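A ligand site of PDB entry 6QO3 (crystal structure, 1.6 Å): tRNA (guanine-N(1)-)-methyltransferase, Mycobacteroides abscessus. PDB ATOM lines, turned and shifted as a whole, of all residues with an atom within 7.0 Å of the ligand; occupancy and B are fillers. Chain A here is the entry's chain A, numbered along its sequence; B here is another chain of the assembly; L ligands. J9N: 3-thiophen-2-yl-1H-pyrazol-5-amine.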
ATOM      1  N   VAL A  84     -18.032  12.073 -15.777  1.00  0.00           N
ATOM      2  CA  VAL A  84     -17.641  10.771 -16.289  1.00  0.00           C
ATOM      3  C   VAL A  84     -18.852  10.017 -16.805  1.00  0.00           C
ATOM      4  O   VAL A  84     -19.598   9.437 -16.010  1.00  0.00           O
ATOM      5  CB  VAL A  84     -16.951   9.909 -15.215  1.00  0.00           C
ATOM      6  CG1 VAL A  84     -16.425   8.625 -15.848  1.00  0.00           C
ATOM      7  CG2 VAL A  84     -15.798  10.664 -14.544  1.00  0.00           C
ATOM      8  N   PRO A  85     -19.076  10.039 -18.125  1.00  0.00           N
ATOM      9  CA  PRO A  85     -20.193   9.255 -18.680  1.00  0.00           C
ATOM     10  C   PRO A  85     -19.998   7.761 -18.438  1.00  0.00           C
ATOM     11  O   PRO A  85     -18.903   7.215 -18.638  1.00  0.00           O
ATOM     12  CB  PRO A  85     -20.158   9.604 -20.171  1.00  0.00           C
ATOM     13  CG  PRO A  85     -19.470  10.944 -20.246  1.00  0.00           C
ATOM     14  CD  PRO A  85     -18.445  10.903 -19.132  1.00  0.00           C
ATOM     15  N   THR A  86     -21.047   7.083 -17.972  1.00  0.00           N
ATOM     16  CA  THR A  86     -21.004   5.639 -17.740  1.00  0.00           C
ATOM     17  C   THR A  86     -22.430   5.109 -17.783  1.00  0.00           C
ATOM     18  O   THR A  86     -23.360   5.805 -17.369  1.00  0.00           O
ATOM     19  CB  THR A  86     -20.339   5.283 -16.390  1.00  0.00           C
ATOM     20  OG1 THR A  86     -20.606   3.910 -16.047  1.00  0.00           O
ATOM     21  CG2 THR A  86     -20.844   6.185 -15.278  1.00  0.00           C
ATOM     22  N   PRO A  87     -22.625   3.901 -18.305  1.00  0.00           N
ATOM     23  CA  PRO A  87     -23.980   3.339 -18.272  1.00  0.00           C
ATOM     24  C   PRO A  87     -24.486   3.156 -16.849  1.00  0.00           C
ATOM     25  O   PRO A  87     -25.704   3.066 -16.635  1.00  0.00           O
ATOM     26  CB  PRO A  87     -23.823   1.967 -18.971  1.00  0.00           C
ATOM     27  CG  PRO A  87     -22.522   2.052 -19.720  1.00  0.00           C
ATOM     28  CD  PRO A  87     -21.652   2.994 -18.937  1.00  0.00           C
ATOM     29  N   ALA A  88     -23.568   3.104 -15.885  1.00  0.00           N
ATOM     30  CA  ALA A  88     -23.942   2.907 -14.486  1.00  0.00           C
ATOM     31  C   ALA A  88     -24.062   4.219 -13.722  1.00  0.00           C
ATOM     32  O   ALA A  88     -24.001   4.223 -12.503  1.00  0.00           O
ATOM     33  CB  ALA A  88     -22.909   1.997 -13.801  1.00  0.00           C
ATOM     34  N   GLY A  89     -24.203   5.331 -14.442  1.00  0.00           N
ATOM     35  CA  GLY A  89     -24.209   6.631 -13.801  1.00  0.00           C
ATOM     36  C   GLY A  89     -25.563   7.060 -13.253  1.00  0.00           C
ATOM     37  O   GLY A  89     -26.583   6.435 -13.501  1.00  0.00           O
ATOM     38  N   ALA A 109     -14.400  12.993 -19.030  1.00  0.00           N
ATOM     39  CA  ALA A 109     -13.520  11.839 -19.234  1.00  0.00           C
ATOM     40  C   ALA A 109     -14.232  10.731 -20.010  1.00  0.00           C
ATOM     41  O   ALA A 109     -15.131  10.066 -19.455  1.00  0.00           O
ATOM     42  CB  ALA A 109     -13.036  11.326 -17.884  1.00  0.00           C
ATOM     43  N   CYS A 110     -13.837  10.517 -21.262  1.00  0.00           N
ATOM     44  CA  CYS A 110     -14.513   9.535 -22.114  1.00  0.00           C
ATOM     45  C   CYS A 110     -13.825   8.193 -22.038  1.00  0.00           C
ATOM     46  O   CYS A 110     -12.644   8.088 -22.395  1.00  0.00           O
ATOM     47  CB  CYS A 110     -14.525   9.995 -23.575  1.00  0.00           C
ATOM     48  SG  CYS A 110     -15.426  11.532 -23.850  1.00  0.00           S
ATOM     49  N   GLY A 111     -14.551   7.165 -21.626  1.00  0.00           N
ATOM     50  CA  GLY A 111     -13.942   5.840 -21.542  1.00  0.00           C
ATOM     51  C   GLY A 111     -14.750   4.760 -22.213  1.00  0.00           C
ATOM     52  O   GLY A 111     -15.876   5.013 -22.660  1.00  0.00           O
ATOM     53  N   ARG A 112     -14.185   3.557 -22.287  1.00  0.00           N
ATOM     54  CA  ARG A 112     -14.914   2.414 -22.842  1.00  0.00           C
ATOM     55  C   ARG A 112     -16.004   1.939 -21.868  1.00  0.00           C
ATOM     56  O   ARG A 112     -15.940   2.231 -20.670  1.00  0.00           O
ATOM     57  CB  ARG A 112     -13.951   1.275 -23.173  1.00  0.00           C
ATOM     58  CG  ARG A 112     -13.098   0.811 -22.006  1.00  0.00           C
ATOM     59  CD  ARG A 112     -12.006  -0.156 -22.480  1.00  0.00           C
ATOM     60  NE  ARG A 112     -12.584  -1.337 -23.131  1.00  0.00           N
ATOM     61  CZ  ARG A 112     -11.978  -2.047 -24.077  1.00  0.00           C
ATOM     62  NH1 ARG A 112     -10.768  -1.709 -24.502  1.00  0.00           N
ATOM     63  NH2 ARG A 112     -12.587  -3.110 -24.595  1.00  0.00           N
ATOM     64  N   TYR A 113     -17.012   1.236 -22.373  1.00  0.00           N
ATOM     65  CA  TYR A 113     -18.179   0.919 -21.534  1.00  0.00           C
ATOM     66  C   TYR A 113     -17.836   0.009 -20.350  1.00  0.00           C
ATOM     67  O   TYR A 113     -18.520   0.066 -19.312  1.00  0.00           O
ATOM     68  CB  TYR A 113     -19.310   0.308 -22.384  1.00  0.00           C
ATOM     69  CG  TYR A 113     -19.130  -1.137 -22.749  1.00  0.00           C
ATOM     70  CD1 TYR A 113     -18.404  -1.512 -23.878  1.00  0.00           C
ATOM     71  CD2 TYR A 113     -19.707  -2.146 -21.983  1.00  0.00           C
ATOM     72  CE1 TYR A 113     -18.247  -2.856 -24.222  1.00  0.00           C
ATOM     73  CE2 TYR A 113     -19.555  -3.474 -22.318  1.00  0.00           C
ATOM     74  CZ  TYR A 113     -18.825  -3.829 -23.437  1.00  0.00           C
ATOM     75  OH  TYR A 113     -18.684  -5.156 -23.758  1.00  0.00           O
ATOM     76  N   GLU A 114     -16.784  -0.807 -20.457  1.00  0.00           N
ATOM     77  CA  GLU A 114     -16.408  -1.681 -19.338  1.00  0.00           C
ATOM     78  C   GLU A 114     -15.869  -0.898 -18.152  1.00  0.00           C
ATOM     79  O   GLU A 114     -15.801  -1.429 -17.041  1.00  0.00           O
ATOM     80  CB  GLU A 114     -15.351  -2.707 -19.771  1.00  0.00           C
ATOM     81  CG  GLU A 114     -15.745  -3.585 -20.935  1.00  0.00           C
ATOM     82  CD  GLU A 114     -15.182  -3.067 -22.237  1.00  0.00           C
ATOM     83  OE1 GLU A 114     -14.802  -3.904 -23.072  1.00  0.00           O
ATOM     84  OE2 GLU A 114     -15.117  -1.835 -22.411  1.00  0.00           O
ATOM     85  N   GLY A 115     -15.459   0.344 -18.389  1.00  0.00           N
ATOM     86  CA  GLY A 115     -15.146   1.254 -17.311  1.00  0.00           C
ATOM     87  C   GLY A 115     -13.715   1.728 -17.207  1.00  0.00           C
ATOM     88  O   GLY A 115     -12.796   1.112 -17.749  1.00  0.00           O
ATOM     89  N   VAL A 133     -22.344   9.908 -14.760  1.00  0.00           N
ATOM     90  CA  VAL A 133     -23.705  10.084 -15.296  1.00  0.00           C
ATOM     91  C   VAL A 133     -24.005   9.214 -16.502  1.00  0.00           C
ATOM     92  O   VAL A 133     -23.146   8.949 -17.342  1.00  0.00           O
ATOM     93  CB  VAL A 133     -23.996  11.567 -15.702  1.00  0.00           C
ATOM     94  CG1 VAL A 133     -24.007  12.487 -14.474  1.00  0.00           C
ATOM     95  CG2 VAL A 133     -23.019  12.078 -16.766  1.00  0.00           C
ATOM     96  N   SER A 134     -25.269   8.807 -16.582  1.00  0.00           N
ATOM     97  CA  SER A 134     -25.819   8.085 -17.712  1.00  0.00           C
ATOM     98  C   SER A 134     -26.706   9.013 -18.533  1.00  0.00           C
ATOM     99  O   SER A 134     -27.412   9.846 -17.951  1.00  0.00           O
ATOM    100  CB  SER A 134     -26.617   6.881 -17.223  1.00  0.00           C
ATOM    101  OG  SER A 134     -27.501   6.401 -18.219  1.00  0.00           O
ATOM    102  N   ILE A 135     -26.686   8.897 -19.866  1.00  0.00           N
ATOM    103  CA  ILE A 135     -27.576   9.734 -20.676  1.00  0.00           C
ATOM    104  C   ILE A 135     -28.836   8.996 -21.144  1.00  0.00           C
ATOM    105  O   ILE A 135     -29.650   9.554 -21.881  1.00  0.00           O
ATOM    106  CB  ILE A 135     -26.847  10.316 -21.910  1.00  0.00           C
ATOM    107  CG1 ILE A 135     -26.335   9.210 -22.846  1.00  0.00           C
ATOM    108  CG2 ILE A 135     -25.707  11.238 -21.479  1.00  0.00           C
ATOM    109  CD1 ILE A 135     -26.084   9.697 -24.282  1.00  0.00           C
ATOM    110  N   GLY A 136     -29.020   7.746 -20.713  1.00  0.00           N
ATOM    111  CA  GLY A 136     -30.230   7.035 -21.071  1.00  0.00           C
ATOM    112  C   GLY A 136     -30.114   5.557 -20.799  1.00  0.00           C
ATOM    113  O   GLY A 136     -29.043   5.058 -20.438  1.00  0.00           O
ATOM    114  N   ASP A 137     -31.233   4.837 -20.958  1.00  0.00           N
ATOM    115  CA  ASP A 137     -31.256   3.420 -20.602  1.00  0.00           C
ATOM    116  C   ASP A 137     -30.887   2.523 -21.762  1.00  0.00           C
ATOM    117  O   ASP A 137     -31.692   1.699 -22.186  1.00  0.00           O
ATOM    118  CB  ASP A 137     -32.630   3.026 -20.070  1.00  0.00           C
ATOM    119  CG  ASP A 137     -32.913   3.602 -18.714  1.00  0.00           C
ATOM    120  OD1 ASP A 137     -31.950   3.894 -17.973  1.00  0.00           O
ATOM    121  OD2 ASP A 137     -34.100   3.762 -18.373  1.00  0.00           O
ATOM    122  N   TYR A 138     -29.677   2.703 -22.269  1.00  0.00           N
ATOM    123  CA  TYR A 138     -29.109   1.896 -23.340  1.00  0.00           C
ATOM    124  C   TYR A 138     -27.606   1.935 -23.143  1.00  0.00           C
ATOM    125  O   TYR A 138     -27.098   2.767 -22.425  1.00  0.00           O
ATOM    126  CB  TYR A 138     -29.468   2.445 -24.721  1.00  0.00           C
ATOM    127  CG  TYR A 138     -29.414   3.956 -24.738  1.00  0.00           C
ATOM    128  CD1 TYR A 138     -28.198   4.635 -24.851  1.00  0.00           C
ATOM    129  CD2 TYR A 138     -30.569   4.695 -24.578  1.00  0.00           C
ATOM    130  CE1 TYR A 138     -28.148   6.021 -24.819  1.00  0.00           C
ATOM    131  CE2 TYR A 138     -30.530   6.083 -24.554  1.00  0.00           C
ATOM    132  CZ  TYR A 138     -29.318   6.742 -24.677  1.00  0.00           C
ATOM    133  OH  TYR A 138     -29.243   8.118 -24.653  1.00  0.00           O
ATOM    134  N   VAL A 139     -26.898   1.005 -23.786  1.00  0.00           N
ATOM    135  CA  VAL A 139     -25.452   0.933 -23.638  1.00  0.00           C
ATOM    136  C   VAL A 139     -24.722   1.353 -24.922  1.00  0.00           C
ATOM    137  O   VAL A 139     -25.011   0.863 -26.012  1.00  0.00           O
ATOM    138  CB  VAL A 139     -25.029  -0.503 -23.236  1.00  0.00           C
ATOM    139  CG1 VAL A 139     -23.510  -0.582 -23.011  1.00  0.00           C
ATOM    140  CG2 VAL A 139     -25.752  -0.910 -21.969  1.00  0.00           C
ATOM    141  N   LEU A 140     -23.781   2.270 -24.773  1.00  0.00           N
ATOM    142  CA  LEU A 140     -22.884   2.672 -25.862  1.00  0.00           C
ATOM    143  C   LEU A 140     -21.570   1.928 -25.705  1.00  0.00           C
ATOM    144  O   LEU A 140     -21.308   1.386 -24.648  1.00  0.00           O
ATOM    145  CB  LEU A 140     -22.642   4.181 -25.825  1.00  0.00           C
ATOM    146  CG  LEU A 140     -23.898   5.037 -25.954  1.00  0.00           C
ATOM    147  CD1 LEU A 140     -23.585   6.496 -25.680  1.00  0.00           C
ATOM    148  CD2 LEU A 140     -24.527   4.855 -27.327  1.00  0.00           C
ATOM    149  N   ASN A 141     -20.736   1.928 -26.733  1.00  0.00           N
ATOM    150  CA  ASN A 141     -19.430   1.275 -26.596  1.00  0.00           C
ATOM    151  C   ASN A 141     -18.410   2.184 -25.917  1.00  0.00           C
ATOM    152  O   ASN A 141     -17.463   1.713 -25.276  1.00  0.00           O
ATOM    153  CB  ASN A 141     -18.900   0.816 -27.947  1.00  0.00           C
ATOM    154  CG  ASN A 141     -18.322  -0.574 -27.893  1.00  0.00           C
ATOM    155  OD1 ASN A 141     -19.026  -1.532 -27.572  1.00  0.00           O
ATOM    156  ND2 ASN A 141     -17.032  -0.703 -28.185  1.00  0.00           N
ATOM    157  N   GLY A 142     -18.590   3.488 -26.068  1.00  0.00           N
ATOM    158  CA  GLY A 142     -17.647   4.456 -25.519  1.00  0.00           C
ATOM    159  C   GLY A 142     -18.341   5.730 -25.096  1.00  0.00           C
ATOM    160  O   GLY A 142     -19.484   5.962 -25.473  1.00  0.00           O
ATOM    161  N   GLY A 143     -17.638   6.572 -24.342  1.00  0.00           N
ATOM    162  CA  GLY A 143     -18.244   7.787 -23.803  1.00  0.00           C
ATOM    163  C   GLY A 143     -18.339   8.976 -24.739  1.00  0.00           C
ATOM    164  O   GLY A 143     -18.992   9.964 -24.401  1.00  0.00           O
ATOM    165  N   GLU A 144     -17.722   8.882 -25.923  1.00  0.00           N
ATOM    166  CA  GLU A 144     -17.667  10.029 -26.843  1.00  0.00           C
ATOM    167  C   GLU A 144     -19.046  10.544 -27.269  1.00  0.00           C
ATOM    168  O   GLU A 144     -19.295  11.750 -27.223  1.00  0.00           O
ATOM    169  CB  GLU A 144     -16.846   9.664 -28.082  1.00  0.00           C
ATOM    170  CG  GLU A 144     -15.337   9.614 -27.829  1.00  0.00           C
ATOM    171  CD  GLU A 144     -14.879   8.364 -27.097  1.00  0.00           C
ATOM    172  OE1 GLU A 144     -15.590   7.334 -27.119  1.00  0.00           O
ATOM    173  OE2 GLU A 144     -13.794   8.417 -26.474  1.00  0.00           O
ATOM    174  N   ALA A 146     -21.851  10.213 -25.691  1.00  0.00           N
ATOM    175  CA  ALA A 146     -22.429  10.806 -24.479  1.00  0.00           C
ATOM    176  C   ALA A 146     -21.851  12.191 -24.210  1.00  0.00           C
ATOM    177  O   ALA A 146     -22.578  13.107 -23.787  1.00  0.00           O
ATOM    178  CB  ALA A 146     -22.216   9.873 -23.267  1.00  0.00           C
ATOM    179  N   GLN B  94     -32.586   0.064 -24.346  1.00  0.00           N
ATOM    180  CA  GLN B  94     -31.777  -1.073 -24.793  1.00  0.00           C
ATOM    181  C   GLN B  94     -32.624  -2.050 -25.586  1.00  0.00           C
ATOM    182  O   GLN B  94     -32.154  -2.662 -26.555  1.00  0.00           O
ATOM    183  CB  GLN B  94     -31.122  -1.776 -23.598  1.00  0.00           C
ATOM    184  CG  GLN B  94     -30.063  -2.811 -24.013  1.00  0.00           C
ATOM    185  CD  GLN B  94     -28.905  -2.180 -24.756  1.00  0.00           C
ATOM    186  OE1 GLN B  94     -28.494  -1.066 -24.447  1.00  0.00           O
ATOM    187  NE2 GLN B  94     -28.371  -2.888 -25.749  1.00  0.00           N
ATOM    188  N   GLU B 152     -24.782   4.097 -32.677  1.00  0.00           N
ATOM    189  CA  GLU B 152     -23.822   3.339 -31.880  1.00  0.00           C
ATOM    190  C   GLU B 152     -24.482   2.253 -31.030  1.00  0.00           C
ATOM    191  O   GLU B 152     -23.990   1.131 -30.951  1.00  0.00           O
ATOM    192  CB  GLU B 152     -23.004   4.266 -30.996  1.00  0.00           C
ATOM    193  CG  GLU B 152     -22.016   3.511 -30.144  1.00  0.00           C
ATOM    194  CD  GLU B 152     -20.934   4.405 -29.573  1.00  0.00           C
ATOM    195  OE1 GLU B 152     -20.894   5.603 -29.954  1.00  0.00           O
ATOM    196  OE2 GLU B 152     -20.144   3.912 -28.752  1.00  0.00           O
HETATM  197  N01 J9N L   1     -26.144   6.092 -20.870  1.00  0.00           N
HETATM  198  C02 J9N L   1     -24.948   5.488 -21.352  1.00  0.00           C
HETATM  199  C03 J9N L   1     -23.621   5.883 -21.150  1.00  0.00           C
HETATM  200  C04 J9N L   1     -22.845   4.944 -21.841  1.00  0.00           C
HETATM  201  C05 J9N L   1     -21.483   4.893 -21.909  1.00  0.00           C
HETATM  202  S06 J9N L   1     -20.426   6.087 -21.269  1.00  0.00           S
HETATM  203  C07 J9N L   1     -18.958   5.282 -21.675  1.00  0.00           C
HETATM  204  C08 J9N L   1     -19.324   4.097 -22.321  1.00  0.00           C
HETATM  205  C09 J9N L   1     -20.692   3.855 -22.438  1.00  0.00           C
HETATM  206  N10 J9N L   1     -23.659   4.065 -22.406  1.00  0.00           N
HETATM  207  N11 J9N L   1     -24.929   4.393 -22.115  1.00  0.00           N
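O of Tyr 138 lies within hydrogen-bond range of N11 of the ligand, 2.7 Å away. N of Leu 140 lies within hydrogen-bond range of N10 of the ligand. OG of Ser 134 is in hydrogen-bond range of N01 of the ligand (3.0 Å). The backbone carbonyl oxygen (O) of Gly 136 lies within hydrogen-bond range of a nitrogen (N01) of the ligand, 3.1 Å away. The backbone NH (N) of Thr 86 sits close to a sulfur (S06) of the ligand, 3.5 Å away.
OH of Tyr 138 lies within hydrogen-bond range of O of Ile 135 (3.1 Å). The side-chain hydroxyl of Ser 134 sits at hydrogen-bond distance from the backbone carbonyl oxygen of Gly 136 (3.0 Å). The backbone carbonyl oxygen (O) of Gly 111 sits at hydrogen-bond distance from the backbone NH (N) of Gly 143 (2.9 Å). N of Gly 142 lies within hydrogen-bond range of OE2 of Glu 152 of chain B, at 3.1 Å. The backbone NH (N) of Tyr 113 is in hydrogen-bond range of the backbone carbonyl oxygen (O) of Asn 141, at 3.0 Å. The backbone carbonyl oxygen (O) of Val 133 sits at hydrogen-bond distance from the backbone NH (N) of Thr 86 (2.9 Å). The backbone NH (N) of Ala 88 sits close to the side-chain hydroxyl (OG1) of Thr 86, at 3.1 Å. OE2 of Glu 114 is in salt-bridge range of NE of Arg 112.
O of Pro 85 sits close to S06 of the ligand, 3.2 Å away. The backbone NH of Ile 135 lies close to a nitrogen (N01) of the ligand (3.0 Å). Merely in contact with the ligand: Pro 87 (3.5 Å), Gly 111 (3.2 Å), Arg 112 (3.99 Å), Tyr 113 (3.5 Å), Val 139 (3.8 Å), Gly 142 (3.4 Å) and Gly 143 (3.2 Å). Hydrophobic or aromatic side chains within 4 Å of the ligand: Pro 85, Pro 87, Tyr 113, Ile 135 and Leu 140.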
